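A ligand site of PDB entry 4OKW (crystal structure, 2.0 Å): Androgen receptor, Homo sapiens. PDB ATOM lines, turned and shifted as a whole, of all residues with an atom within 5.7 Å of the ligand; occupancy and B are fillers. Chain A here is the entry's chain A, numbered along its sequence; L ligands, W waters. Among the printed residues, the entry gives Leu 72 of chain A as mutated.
Water W1 lies within hydrogen-bond range of NE2 of His 205 (2.8 Å), O of Gln 69 (2.9 Å), N of Met 73 (2.9 Å) and N of Leu 72 (3.4 Å).
Water W2 lies within hydrogen-bond range of NE2 of Gln 42 (2.8 Å), O of Met 76 (2.8 Å), NH2 of Arg 83 (3.0 Å) and N2 of the ligand (3.2 Å).
SD of Met 73 sits close to O4 of the ligand (3.5 Å).
N of Val 77 sits close to F2 of the ligand (3.3 Å).
The side-chain sulfur of Met 118 lies close to a fluorine (F4) of the ligand (3.7 Å).
Merely in contact with the ligand: Leu 38 (3.6 Å), Gly 39 (3.5 Å), Gln 69 (3.8 Å), Leu 72 (3.8 Å), Met 76 (3.3 Å), Met 80 (3.4 Å), Phe 95 (3.5 Å), Leu 204 (3.7 Å), His 205 (3.8 Å), Thr 208 (3.4 Å), Met 226 (3.5 Å), Ile 229 (3.5 Å), Ile 230 (3.6 Å) and Val 234 (3.3 Å).
Hydrophobic or aromatic side chains that line the ligand: Leu 35, Leu 38, Leu 72, Met 73, Met 76, Val 77, Met 80, Phe 95, Met 118, Leu 204, Met 226, Ile 229, Ile 230 and Val 234.
21 residues have an atom within 4 Å of the ligand: Leu 35, Asn 36, Leu 38, Gly 39, Gln 42, Gln 69, Leu 72, Met 73, Met 76, Val 77, Met 80, Arg 83, Phe 95, Met 118, Leu 204, His 205, Thr 208, Met 226, Ile 229, Ile 230 and Val 234.
The nearest printed residue that does not touch the ligand is Phe 207 (4.6 Å).
O3 of the ligand lies within hydrogen-bond range of O of Leu 35 (3.1 Å).
OD1 of Asn 36 is in hydrogen-bond range of O3 of the ligand.
OE1 of Gln 42 lies close to N2 of the ligand (3.4 Å).
The backbone NH (N) of Asn 36 sits close to an oxygen (O3) of the ligand (3.2 Å).
N2 of the ligand is in hydrogen-bond range of NH2 of Arg 83, 2.9 Å away.
NE2 of Gln 42 lies close to SD of Met 76, 3.4 Å away.
The guanidinium group (NH2) of Arg 83 is in hydrogen-bond range of the backbone carbonyl oxygen (O) of Phe 95 (2.9 Å).
N of Val 234 lies within hydrogen-bond range of O of Ile 229, at 3.1 Å.
OG1 of Thr 208 sits at hydrogen-bond distance from O of Leu 204, 2.9 Å away.
The guanidinium group (NE) of Arg 83 lies within hydrogen-bond range of the backbone carbonyl oxygen (O) of Tyr 94, at 3.0 Å.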
ATOM      1  N   LEU A  32      -8.940  -8.706  10.314  1.00  0.00           N
ATOM      2  CA  LEU A  32      -9.193  -9.859   9.457  1.00  0.00           C
ATOM      3  C   LEU A  32      -8.513  -9.661   8.109  1.00  0.00           C
ATOM      4  O   LEU A  32      -7.657 -10.466   7.723  1.00  0.00           O
ATOM      5  CB  LEU A  32     -10.695 -10.056   9.257  1.00  0.00           C
ATOM      6  CG  LEU A  32     -11.334 -11.187  10.078  1.00  0.00           C
ATOM      7  CD1 LEU A  32     -11.104 -10.963  11.565  1.00  0.00           C
ATOM      8  CD2 LEU A  32     -12.817 -11.293   9.766  1.00  0.00           C
ATOM      9  N   LEU A  35      -4.990 -10.292   8.484  1.00  0.00           N
ATOM     10  CA  LEU A  35      -4.619 -11.695   8.718  1.00  0.00           C
ATOM     11  C   LEU A  35      -4.654 -12.484   7.405  1.00  0.00           C
ATOM     12  O   LEU A  35      -3.895 -13.442   7.241  1.00  0.00           O
ATOM     13  CB  LEU A  35      -5.518 -12.371   9.798  1.00  0.00           C
ATOM     14  CG  LEU A  35      -5.119 -12.064  11.240  1.00  0.00           C
ATOM     15  CD1 LEU A  35      -6.189 -12.576  12.241  1.00  0.00           C
ATOM     16  CD2 LEU A  35      -3.743 -12.686  11.538  1.00  0.00           C
ATOM     17  N   ASN A  36      -5.629 -12.170   6.525  1.00  0.00           N
ATOM     18  CA  ASN A  36      -5.818 -12.908   5.291  1.00  0.00           C
ATOM     19  C   ASN A  36      -4.666 -12.588   4.360  1.00  0.00           C
ATOM     20  O   ASN A  36      -4.156 -13.446   3.647  1.00  0.00           O
ATOM     21  CB  ASN A  36      -7.130 -12.487   4.591  1.00  0.00           C
ATOM     22  CG  ASN A  36      -8.362 -12.910   5.362  1.00  0.00           C
ATOM     23  OD1 ASN A  36      -8.333 -13.901   6.132  1.00  0.00           O
ATOM     24  ND2 ASN A  36      -9.498 -12.225   5.090  1.00  0.00           N
ATOM     25  N   GLU A  37      -4.292 -11.321   4.327  1.00  0.00           N
ATOM     26  CA  GLU A  37      -3.147 -10.919   3.514  1.00  0.00           C
ATOM     27  C   GLU A  37      -1.874 -11.597   4.065  1.00  0.00           C
ATOM     28  O   GLU A  37      -1.099 -12.147   3.323  1.00  0.00           O
ATOM     29  CB  GLU A  37      -3.009  -9.405   3.444  1.00  0.00           C
ATOM     30  CG  GLU A  37      -1.696  -8.911   2.850  1.00  0.00           C
ATOM     31  CD  GLU A  37      -1.562  -9.257   1.353  1.00  0.00           C
ATOM     32  OE1 GLU A  37      -0.413  -9.379   0.860  1.00  0.00           O
ATOM     33  OE2 GLU A  37      -2.594  -9.435   0.688  1.00  0.00           O
ATOM     34  N   LEU A  38      -1.691 -11.575   5.388  1.00  0.00           N
ATOM     35  CA  LEU A  38      -0.573 -12.261   5.998  1.00  0.00           C
ATOM     36  C   LEU A  38      -0.588 -13.745   5.664  1.00  0.00           C
ATOM     37  O   LEU A  38       0.445 -14.357   5.407  1.00  0.00           O
ATOM     38  CB  LEU A  38      -0.565 -12.049   7.517  1.00  0.00           C
ATOM     39  CG  LEU A  38       0.617 -12.674   8.256  1.00  0.00           C
ATOM     40  CD1 LEU A  38       1.967 -12.091   7.698  1.00  0.00           C
ATOM     41  CD2 LEU A  38       0.439 -12.436   9.768  1.00  0.00           C
ATOM     42  N   GLY A  39      -1.766 -14.336   5.653  1.00  0.00           N
ATOM     43  CA  GLY A  39      -1.772 -15.784   5.360  1.00  0.00           C
ATOM     44  C   GLY A  39      -1.251 -16.043   3.960  1.00  0.00           C
ATOM     45  O   GLY A  39      -0.559 -17.002   3.723  1.00  0.00           O
ATOM     46  N   GLU A  40      -1.596 -15.203   3.000  1.00  0.00           N
ATOM     47  CA  GLU A  40      -1.068 -15.454   1.650  1.00  0.00           C
ATOM     48  C   GLU A  40       0.442 -15.284   1.596  1.00  0.00           C
ATOM     49  O   GLU A  40       1.141 -16.043   0.897  1.00  0.00           O
ATOM     50  CB  GLU A  40      -1.668 -14.489   0.617  1.00  0.00           C
ATOM     51  CG  GLU A  40      -1.223 -14.871  -0.789  1.00  0.00           C
ATOM     52  CD  GLU A  40      -1.983 -14.104  -1.816  1.00  0.00           C
ATOM     53  OE1 GLU A  40      -2.714 -14.764  -2.568  1.00  0.00           O
ATOM     54  OE2 GLU A  40      -1.933 -12.855  -1.811  1.00  0.00           O
ATOM     55  N   GLN A  42       2.578 -15.651   4.028  1.00  0.00           N
ATOM     56  CA  GLN A  42       3.221 -16.788   4.646  1.00  0.00           C
ATOM     57  C   GLN A  42       3.110 -18.039   3.749  1.00  0.00           C
ATOM     58  O   GLN A  42       4.035 -18.798   3.661  1.00  0.00           O
ATOM     59  CB  GLN A  42       2.673 -17.068   6.084  1.00  0.00           C
ATOM     60  CG  GLN A  42       2.970 -15.909   7.060  1.00  0.00           C
ATOM     61  CD  GLN A  42       2.714 -16.234   8.543  1.00  0.00           C
ATOM     62  OE1 GLN A  42       2.913 -15.374   9.450  1.00  0.00           O
ATOM     63  NE2 GLN A  42       2.301 -17.453   8.804  1.00  0.00           N
ATOM     64  N   GLN A  69      -1.186 -27.264   1.148  1.00  0.00           N
ATOM     65  CA  GLN A  69      -2.448 -26.613   1.408  1.00  0.00           C
ATOM     66  C   GLN A  69      -3.197 -27.162   2.662  1.00  0.00           C
ATOM     67  O   GLN A  69      -3.751 -26.379   3.432  1.00  0.00           O
ATOM     68  CB  GLN A  69      -3.325 -26.784   0.163  1.00  0.00           C
ATOM     69  CG  GLN A  69      -2.865 -25.856  -0.969  1.00  0.00           C
ATOM     70  CD  GLN A  69      -3.556 -26.244  -2.238  1.00  0.00           C
ATOM     71  OE1 GLN A  69      -3.247 -27.274  -2.860  1.00  0.00           O
ATOM     72  NE2 GLN A  69      -4.576 -25.514  -2.561  1.00  0.00           N
ATOM     73  N   LEU A  72      -1.093 -25.996   5.834  1.00  0.00           N
ATOM     74  CA  LEU A  72      -0.680 -24.618   5.979  1.00  0.00           C
ATOM     75  C   LEU A  72      -1.137 -24.043   7.350  1.00  0.00           C
ATOM     76  O   LEU A  72      -0.372 -23.383   8.009  1.00  0.00           O
ATOM     77  CB  LEU A  72      -1.325 -23.725   4.840  1.00  0.00           C
ATOM     78  CG  LEU A  72      -1.120 -22.228   5.034  1.00  0.00           C
ATOM     79  CD1 LEU A  72       0.365 -21.875   4.922  1.00  0.00           C
ATOM     80  CD2 LEU A  72      -1.877 -21.404   3.989  1.00  0.00           C
ATOM     81  N   MET A  73      -2.423 -24.230   7.723  1.00  0.00           N
ATOM     82  CA  MET A  73      -2.886 -23.598   8.973  1.00  0.00           C
ATOM     83  C   MET A  73      -2.027 -24.019  10.190  1.00  0.00           C
ATOM     84  O   MET A  73      -1.607 -23.155  11.001  1.00  0.00           O
ATOM     85  CB  MET A  73      -4.398 -23.898   9.229  1.00  0.00           C
ATOM     86  CG  MET A  73      -5.024 -23.054  10.400  1.00  0.00           C
ATOM     87  SD  MET A  73      -5.059 -21.288   9.978  1.00  0.00           S
ATOM     88  CE  MET A  73      -6.601 -21.280   9.038  1.00  0.00           C
ATOM     89  N   MET A  76       1.388 -22.562  10.235  1.00  0.00           N
ATOM     90  CA  MET A  76       1.400 -21.131  10.540  1.00  0.00           C
ATOM     91  C   MET A  76       1.171 -20.962  12.079  1.00  0.00           C
ATOM     92  O   MET A  76       1.823 -20.124  12.706  1.00  0.00           O
ATOM     93  CB  MET A  76       0.306 -20.398   9.794  1.00  0.00           C
ATOM     94  CG  MET A  76       0.563 -20.278   8.225  1.00  0.00           C
ATOM     95  SD  MET A  76      -0.460 -18.942   7.579  1.00  0.00           S
ATOM     96  CE  MET A  76      -2.085 -19.552   7.883  1.00  0.00           C
ATOM     97  N   VAL A  77       0.324 -21.822  12.665  1.00  0.00           N
ATOM     98  CA  VAL A  77       0.004 -21.708  14.099  1.00  0.00           C
ATOM     99  C   VAL A  77       1.247 -22.082  14.882  1.00  0.00           C
ATOM    100  O   VAL A  77       1.611 -21.402  15.814  1.00  0.00           O
ATOM    101  CB  VAL A  77      -1.137 -22.686  14.482  1.00  0.00           C
ATOM    102  CG1 VAL A  77      -1.186 -22.888  15.998  1.00  0.00           C
ATOM    103  CG2 VAL A  77      -2.459 -22.165  13.910  1.00  0.00           C
ATOM    104  N   MET A  80       3.872 -19.532  14.570  1.00  0.00           N
ATOM    105  CA  MET A  80       3.452 -18.298  15.256  1.00  0.00           C
ATOM    106  C   MET A  80       3.672 -18.491  16.759  1.00  0.00           C
ATOM    107  O   MET A  80       4.109 -17.541  17.445  1.00  0.00           O
ATOM    108  CB  MET A  80       2.006 -17.936  14.971  1.00  0.00           C
ATOM    109  CG  MET A  80       1.600 -16.550  15.438  1.00  0.00           C
ATOM    110  SD  MET A  80       1.052 -16.572  17.193  1.00  0.00           S
ATOM    111  CE  MET A  80      -0.655 -17.161  17.002  1.00  0.00           C
ATOM    112  N   ARG A  83       7.321 -17.916  17.470  1.00  0.00           N
ATOM    113  CA  ARG A  83       7.632 -16.442  17.428  1.00  0.00           C
ATOM    114  C   ARG A  83       7.169 -15.711  18.649  1.00  0.00           C
ATOM    115  O   ARG A  83       7.936 -14.840  19.207  1.00  0.00           O
ATOM    116  CB  ARG A  83       6.993 -15.717  16.219  1.00  0.00           C
ATOM    117  CG  ARG A  83       7.688 -15.944  14.945  1.00  0.00           C
ATOM    118  CD  ARG A  83       7.229 -14.960  13.852  1.00  0.00           C
ATOM    119  NE  ARG A  83       5.796 -15.050  13.603  1.00  0.00           N
ATOM    120  CZ  ARG A  83       5.203 -16.021  12.898  1.00  0.00           C
ATOM    121  NH1 ARG A  83       5.921 -17.018  12.371  1.00  0.00           N
ATOM    122  NH2 ARG A  83       3.899 -15.992  12.754  1.00  0.00           N
ATOM    123  N   TYR A  94       2.382 -13.028  18.306  1.00  0.00           N
ATOM    124  CA  TYR A  94       3.227 -12.315  17.370  1.00  0.00           C
ATOM    125  C   TYR A  94       2.990 -12.881  15.948  1.00  0.00           C
ATOM    126  O   TYR A  94       3.812 -13.619  15.421  1.00  0.00           O
ATOM    127  CB  TYR A  94       4.645 -12.498  17.843  1.00  0.00           C
ATOM    128  CG  TYR A  94       5.647 -11.526  17.278  1.00  0.00           C
ATOM    129  CD1 TYR A  94       6.121 -10.444  18.047  1.00  0.00           C
ATOM    130  CD2 TYR A  94       6.150 -11.717  15.979  1.00  0.00           C
ATOM    131  CE1 TYR A  94       7.101  -9.567  17.521  1.00  0.00           C
ATOM    132  CE2 TYR A  94       7.103 -10.831  15.431  1.00  0.00           C
ATOM    133  CZ  TYR A  94       7.585  -9.785  16.202  1.00  0.00           C
ATOM    134  OH  TYR A  94       8.547  -8.967  15.614  1.00  0.00           O
ATOM    135  N   PHE A  95       1.876 -12.503  15.349  1.00  0.00           N
ATOM    136  CA  PHE A  95       1.554 -12.998  14.006  1.00  0.00           C
ATOM    137  C   PHE A  95       2.638 -12.471  13.044  1.00  0.00           C
ATOM    138  O   PHE A  95       3.192 -13.230  12.251  1.00  0.00           O
ATOM    139  CB  PHE A  95       0.212 -12.480  13.594  1.00  0.00           C
ATOM    140  CG  PHE A  95      -0.944 -13.164  14.270  1.00  0.00           C
ATOM    141  CD1 PHE A  95      -1.553 -12.566  15.326  1.00  0.00           C
ATOM    142  CD2 PHE A  95      -1.421 -14.398  13.822  1.00  0.00           C
ATOM    143  CE1 PHE A  95      -2.624 -13.212  15.995  1.00  0.00           C
ATOM    144  CE2 PHE A  95      -2.529 -15.013  14.450  1.00  0.00           C
ATOM    145  CZ  PHE A  95      -3.105 -14.433  15.544  1.00  0.00           C
ATOM    146  N   MET A 111     -11.831 -13.961  17.455  1.00  0.00           N
ATOM    147  CA  MET A 111     -11.084 -15.210  17.447  1.00  0.00           C
ATOM    148  C   MET A 111     -10.543 -15.494  18.818  1.00  0.00           C
ATOM    149  O   MET A 111      -9.512 -16.125  18.953  1.00  0.00           O
ATOM    150  CB  MET A 111      -9.887 -15.085  16.502  1.00  0.00           C
ATOM    151  CG  MET A 111     -10.199 -14.957  15.030  1.00  0.00           C
ATOM    152  SD  MET A 111      -8.682 -14.581  14.104  1.00  0.00           S
ATOM    153  CE  MET A 111      -7.741 -15.994  14.664  1.00  0.00           C
ATOM    154  N   MET A 118      -3.938 -20.646  21.192  1.00  0.00           N
ATOM    155  CA  MET A 118      -2.612 -20.424  20.589  1.00  0.00           C
ATOM    156  C   MET A 118      -1.614 -19.877  21.594  1.00  0.00           C
ATOM    157  O   MET A 118      -0.454 -20.272  21.613  1.00  0.00           O
ATOM    158  CB  MET A 118      -2.763 -19.521  19.363  1.00  0.00           C
ATOM    159  CG  MET A 118      -3.537 -20.248  18.257  1.00  0.00           C
ATOM    160  SD  MET A 118      -3.399 -19.396  16.683  1.00  0.00           S
ATOM    161  CE  MET A 118      -4.582 -18.061  16.764  1.00  0.00           C
ATOM    162  N   LEU A 204      -9.601 -22.898  13.584  1.00  0.00           N
ATOM    163  CA  LEU A 204      -9.295 -21.771  12.717  1.00  0.00           C
ATOM    164  C   LEU A 204      -9.816 -22.010  11.329  1.00  0.00           C
ATOM    165  O   LEU A 204     -10.278 -21.077  10.683  1.00  0.00           O
ATOM    166  CB  LEU A 204      -7.752 -21.594  12.680  1.00  0.00           C
ATOM    167  CG  LEU A 204      -7.208 -20.897  13.964  1.00  0.00           C
ATOM    168  CD1 LEU A 204      -5.685 -20.910  14.009  1.00  0.00           C
ATOM    169  CD2 LEU A 204      -7.740 -19.474  14.102  1.00  0.00           C
ATOM    170  N   HIS A 205      -9.664 -23.246  10.826  1.00  0.00           N
ATOM    171  CA  HIS A 205     -10.268 -23.551   9.513  1.00  0.00           C
ATOM    172  C   HIS A 205     -11.785 -23.371   9.544  1.00  0.00           C
ATOM    173  O   HIS A 205     -12.357 -22.922   8.544  1.00  0.00           O
ATOM    174  CB  HIS A 205     -10.075 -25.009   9.102  1.00  0.00           C
ATOM    175  CG  HIS A 205      -8.722 -25.319   8.558  1.00  0.00           C
ATOM    176  ND1 HIS A 205      -8.030 -26.435   8.970  1.00  0.00           N
ATOM    177  CD2 HIS A 205      -7.966 -24.718   7.614  1.00  0.00           C
ATOM    178  CE1 HIS A 205      -6.899 -26.515   8.281  1.00  0.00           C
ATOM    179  NE2 HIS A 205      -6.843 -25.490   7.454  1.00  0.00           N
ATOM    180  N   PHE A 207     -13.499 -21.292  11.468  1.00  0.00           N
ATOM    181  CA  PHE A 207     -13.749 -19.832  11.544  1.00  0.00           C
ATOM    182  C   PHE A 207     -13.497 -19.176  10.194  1.00  0.00           C
ATOM    183  O   PHE A 207     -14.223 -18.258   9.733  1.00  0.00           O
ATOM    184  CB  PHE A 207     -12.845 -19.212  12.644  1.00  0.00           C
ATOM    185  CG  PHE A 207     -12.704 -17.702  12.582  1.00  0.00           C
ATOM    186  CD1 PHE A 207     -11.799 -17.086  11.727  1.00  0.00           C
ATOM    187  CD2 PHE A 207     -13.465 -16.880  13.419  1.00  0.00           C
ATOM    188  CE1 PHE A 207     -11.654 -15.697  11.694  1.00  0.00           C
ATOM    189  CE2 PHE A 207     -13.354 -15.489  13.374  1.00  0.00           C
ATOM    190  CZ  PHE A 207     -12.425 -14.890  12.514  1.00  0.00           C
ATOM    191  N   THR A 208     -12.413 -19.632   9.541  1.00  0.00           N
ATOM    192  CA  THR A 208     -12.011 -19.091   8.221  1.00  0.00           C
ATOM    193  C   THR A 208     -13.050 -19.354   7.098  1.00  0.00           C
ATOM    194  O   THR A 208     -13.338 -18.473   6.260  1.00  0.00           O
ATOM    195  CB  THR A 208     -10.625 -19.672   7.769  1.00  0.00           C
ATOM    196  OG1 THR A 208      -9.563 -19.168   8.624  1.00  0.00           O
ATOM    197  CG2 THR A 208     -10.311 -19.270   6.309  1.00  0.00           C
ATOM    198  N   LEU A 211     -16.139 -17.286   7.732  1.00  0.00           N
ATOM    199  CA  LEU A 211     -15.856 -15.901   7.438  1.00  0.00           C
ATOM    200  C   LEU A 211     -15.874 -15.621   5.951  1.00  0.00           C
ATOM    201  O   LEU A 211     -16.319 -14.564   5.496  1.00  0.00           O
ATOM    202  CB  LEU A 211     -14.471 -15.491   8.005  1.00  0.00           C
ATOM    203  CG  LEU A 211     -13.975 -14.038   7.760  1.00  0.00           C
ATOM    204  CD1 LEU A 211     -15.033 -13.053   8.250  1.00  0.00           C
ATOM    205  CD2 LEU A 211     -12.626 -13.802   8.458  1.00  0.00           C
ATOM    206  N   PHE A 222     -10.495 -11.091   1.097  1.00  0.00           N
ATOM    207  CA  PHE A 222      -9.623 -12.299   0.927  1.00  0.00           C
ATOM    208  C   PHE A 222      -8.876 -12.216  -0.388  1.00  0.00           C
ATOM    209  O   PHE A 222      -9.500 -12.095  -1.476  1.00  0.00           O
ATOM    210  CB  PHE A 222     -10.391 -13.606   0.880  1.00  0.00           C
ATOM    211  CG  PHE A 222     -10.948 -14.035   2.193  1.00  0.00           C
ATOM    212  CD1 PHE A 222     -12.159 -13.537   2.625  1.00  0.00           C
ATOM    213  CD2 PHE A 222     -10.232 -14.913   3.021  1.00  0.00           C
ATOM    214  CE1 PHE A 222     -12.701 -13.900   3.887  1.00  0.00           C
ATOM    215  CE2 PHE A 222     -10.762 -15.303   4.253  1.00  0.00           C
ATOM    216  CZ  PHE A 222     -12.005 -14.807   4.682  1.00  0.00           C
ATOM    217  N   MET A 226      -6.298 -17.349  -1.533  1.00  0.00           N
ATOM    218  CA  MET A 226      -6.757 -17.797  -0.226  1.00  0.00           C
ATOM    219  C   MET A 226      -8.264 -18.153  -0.333  1.00  0.00           C
ATOM    220  O   MET A 226      -8.659 -19.177   0.157  1.00  0.00           O
ATOM    221  CB  MET A 226      -6.474 -16.758   0.855  1.00  0.00           C
ATOM    222  CG  MET A 226      -4.985 -16.366   0.916  1.00  0.00           C
ATOM    223  SD  MET A 226      -3.783 -17.719   0.749  1.00  0.00           S
ATOM    224  CE  MET A 226      -3.914 -18.330   2.450  1.00  0.00           C
ATOM    225  N   ILE A 229      -8.367 -21.625  -1.992  1.00  0.00           N
ATOM    226  CA  ILE A 229      -7.986 -22.638  -1.007  1.00  0.00           C
ATOM    227  C   ILE A 229      -9.113 -22.878  -0.007  1.00  0.00           C
ATOM    228  O   ILE A 229      -9.416 -24.001   0.294  1.00  0.00           O
ATOM    229  CB  ILE A 229      -6.650 -22.287  -0.290  1.00  0.00           C
ATOM    230  CG1 ILE A 229      -5.524 -22.342  -1.343  1.00  0.00           C
ATOM    231  CG2 ILE A 229      -6.307 -23.277   0.849  1.00  0.00           C
ATOM    232  CD1 ILE A 229      -4.216 -21.674  -0.896  1.00  0.00           C
ATOM    233  N   ILE A 230      -9.718 -21.823   0.525  1.00  0.00           N
ATOM    234  CA  ILE A 230     -10.745 -21.970   1.508  1.00  0.00           C
ATOM    235  C   ILE A 230     -11.965 -22.698   0.904  1.00  0.00           C
ATOM    236  O   ILE A 230     -12.560 -23.537   1.572  1.00  0.00           O
ATOM    237  CB  ILE A 230     -11.137 -20.612   2.168  1.00  0.00           C
ATOM    238  CG1 ILE A 230      -9.871 -19.972   2.792  1.00  0.00           C
ATOM    239  CG2 ILE A 230     -12.202 -20.818   3.261  1.00  0.00           C
ATOM    240  CD1 ILE A 230      -9.962 -18.464   3.042  1.00  0.00           C
ATOM    241  N   VAL A 234     -10.108 -26.484   2.024  1.00  0.00           N
ATOM    242  CA  VAL A 234     -10.482 -26.456   3.453  1.00  0.00           C
ATOM    243  C   VAL A 234     -11.800 -27.307   3.738  1.00  0.00           C
ATOM    244  O   VAL A 234     -11.858 -27.954   4.757  1.00  0.00           O
ATOM    245  CB  VAL A 234     -10.610 -24.988   3.943  1.00  0.00           C
ATOM    246  CG1 VAL A 234     -11.398 -24.864   5.253  1.00  0.00           C
ATOM    247  CG2 VAL A 234      -9.198 -24.323   4.118  1.00  0.00           C
HETATM  248  C1  LIG L   1      -5.156 -20.316   6.204  1.00  0.00           C
HETATM  249  C2  LIG L   1      -5.176 -21.684   5.829  1.00  0.00           C
HETATM  250  C3  LIG L   1      -5.940 -22.134   4.751  1.00  0.00           C
HETATM  251  F1  LIG L   1      -6.021 -23.438   4.312  1.00  0.00           F
HETATM  252  C4  LIG L   1      -6.655 -21.210   3.983  1.00  0.00           C
HETATM  253  C5  LIG L   1      -6.662 -19.883   4.381  1.00  0.00           C
HETATM  254  C6  LIG L   1      -5.915 -19.371   5.450  1.00  0.00           C
HETATM  255  S1  LIG L   1      -6.039 -17.729   5.701  1.00  0.00           S
HETATM  256  O1  LIG L   1      -4.769 -17.332   6.146  1.00  0.00           O
HETATM  257  O2  LIG L   1      -6.445 -17.023   4.477  1.00  0.00           O
HETATM  258  C7  LIG L   1      -7.281 -17.376   6.858  1.00  0.00           C
HETATM  259  C8  LIG L   1      -6.922 -16.335   7.951  1.00  0.00           C
HETATM  260  O3  LIG L   1      -6.534 -15.100   7.316  1.00  0.00           O
HETATM  261  C9  LIG L   1      -8.076 -15.961   8.889  1.00  0.00           C
HETATM  262  C10 LIG L   1      -5.758 -16.801   8.853  1.00  0.00           C
HETATM  263  O4  LIG L   1      -5.821 -17.882   9.415  1.00  0.00           O
HETATM  264  N1  LIG L   1      -4.686 -15.992   8.863  1.00  0.00           N
HETATM  265  C11 LIG L   1      -3.502 -16.252   9.537  1.00  0.00           C
HETATM  266  C12 LIG L   1      -3.421 -17.162  10.618  1.00  0.00           C
HETATM  267  C13 LIG L   1      -2.391 -15.510   9.191  1.00  0.00           C
HETATM  268  C14 LIG L   1      -1.152 -15.632   9.839  1.00  0.00           C
HETATM  269  C15 LIG L   1      -1.032 -16.565  10.870  1.00  0.00           C
HETATM  270  C16 LIG L   1       0.104 -16.573  11.460  1.00  0.00           C
HETATM  271  N2  LIG L   1       1.114 -16.558  12.021  1.00  0.00           N
HETATM  272  C17 LIG L   1      -2.216 -17.318  11.318  1.00  0.00           C
HETATM  273  C18 LIG L   1      -2.152 -18.314  12.464  1.00  0.00           C
HETATM  274  F2  LIG L   1      -1.963 -19.510  12.041  1.00  0.00           F
HETATM  275  F3  LIG L   1      -1.148 -18.108  13.236  1.00  0.00           F
HETATM  276  F4  LIG L   1      -3.226 -18.257  13.205  1.00  0.00           F
HETATM  277  O   HOH W   1      -4.410 -25.466   6.058  1.00  0.00           O
HETATM  278  O   HOH W   2       3.513 -18.447  11.145  1.00  0.00           O
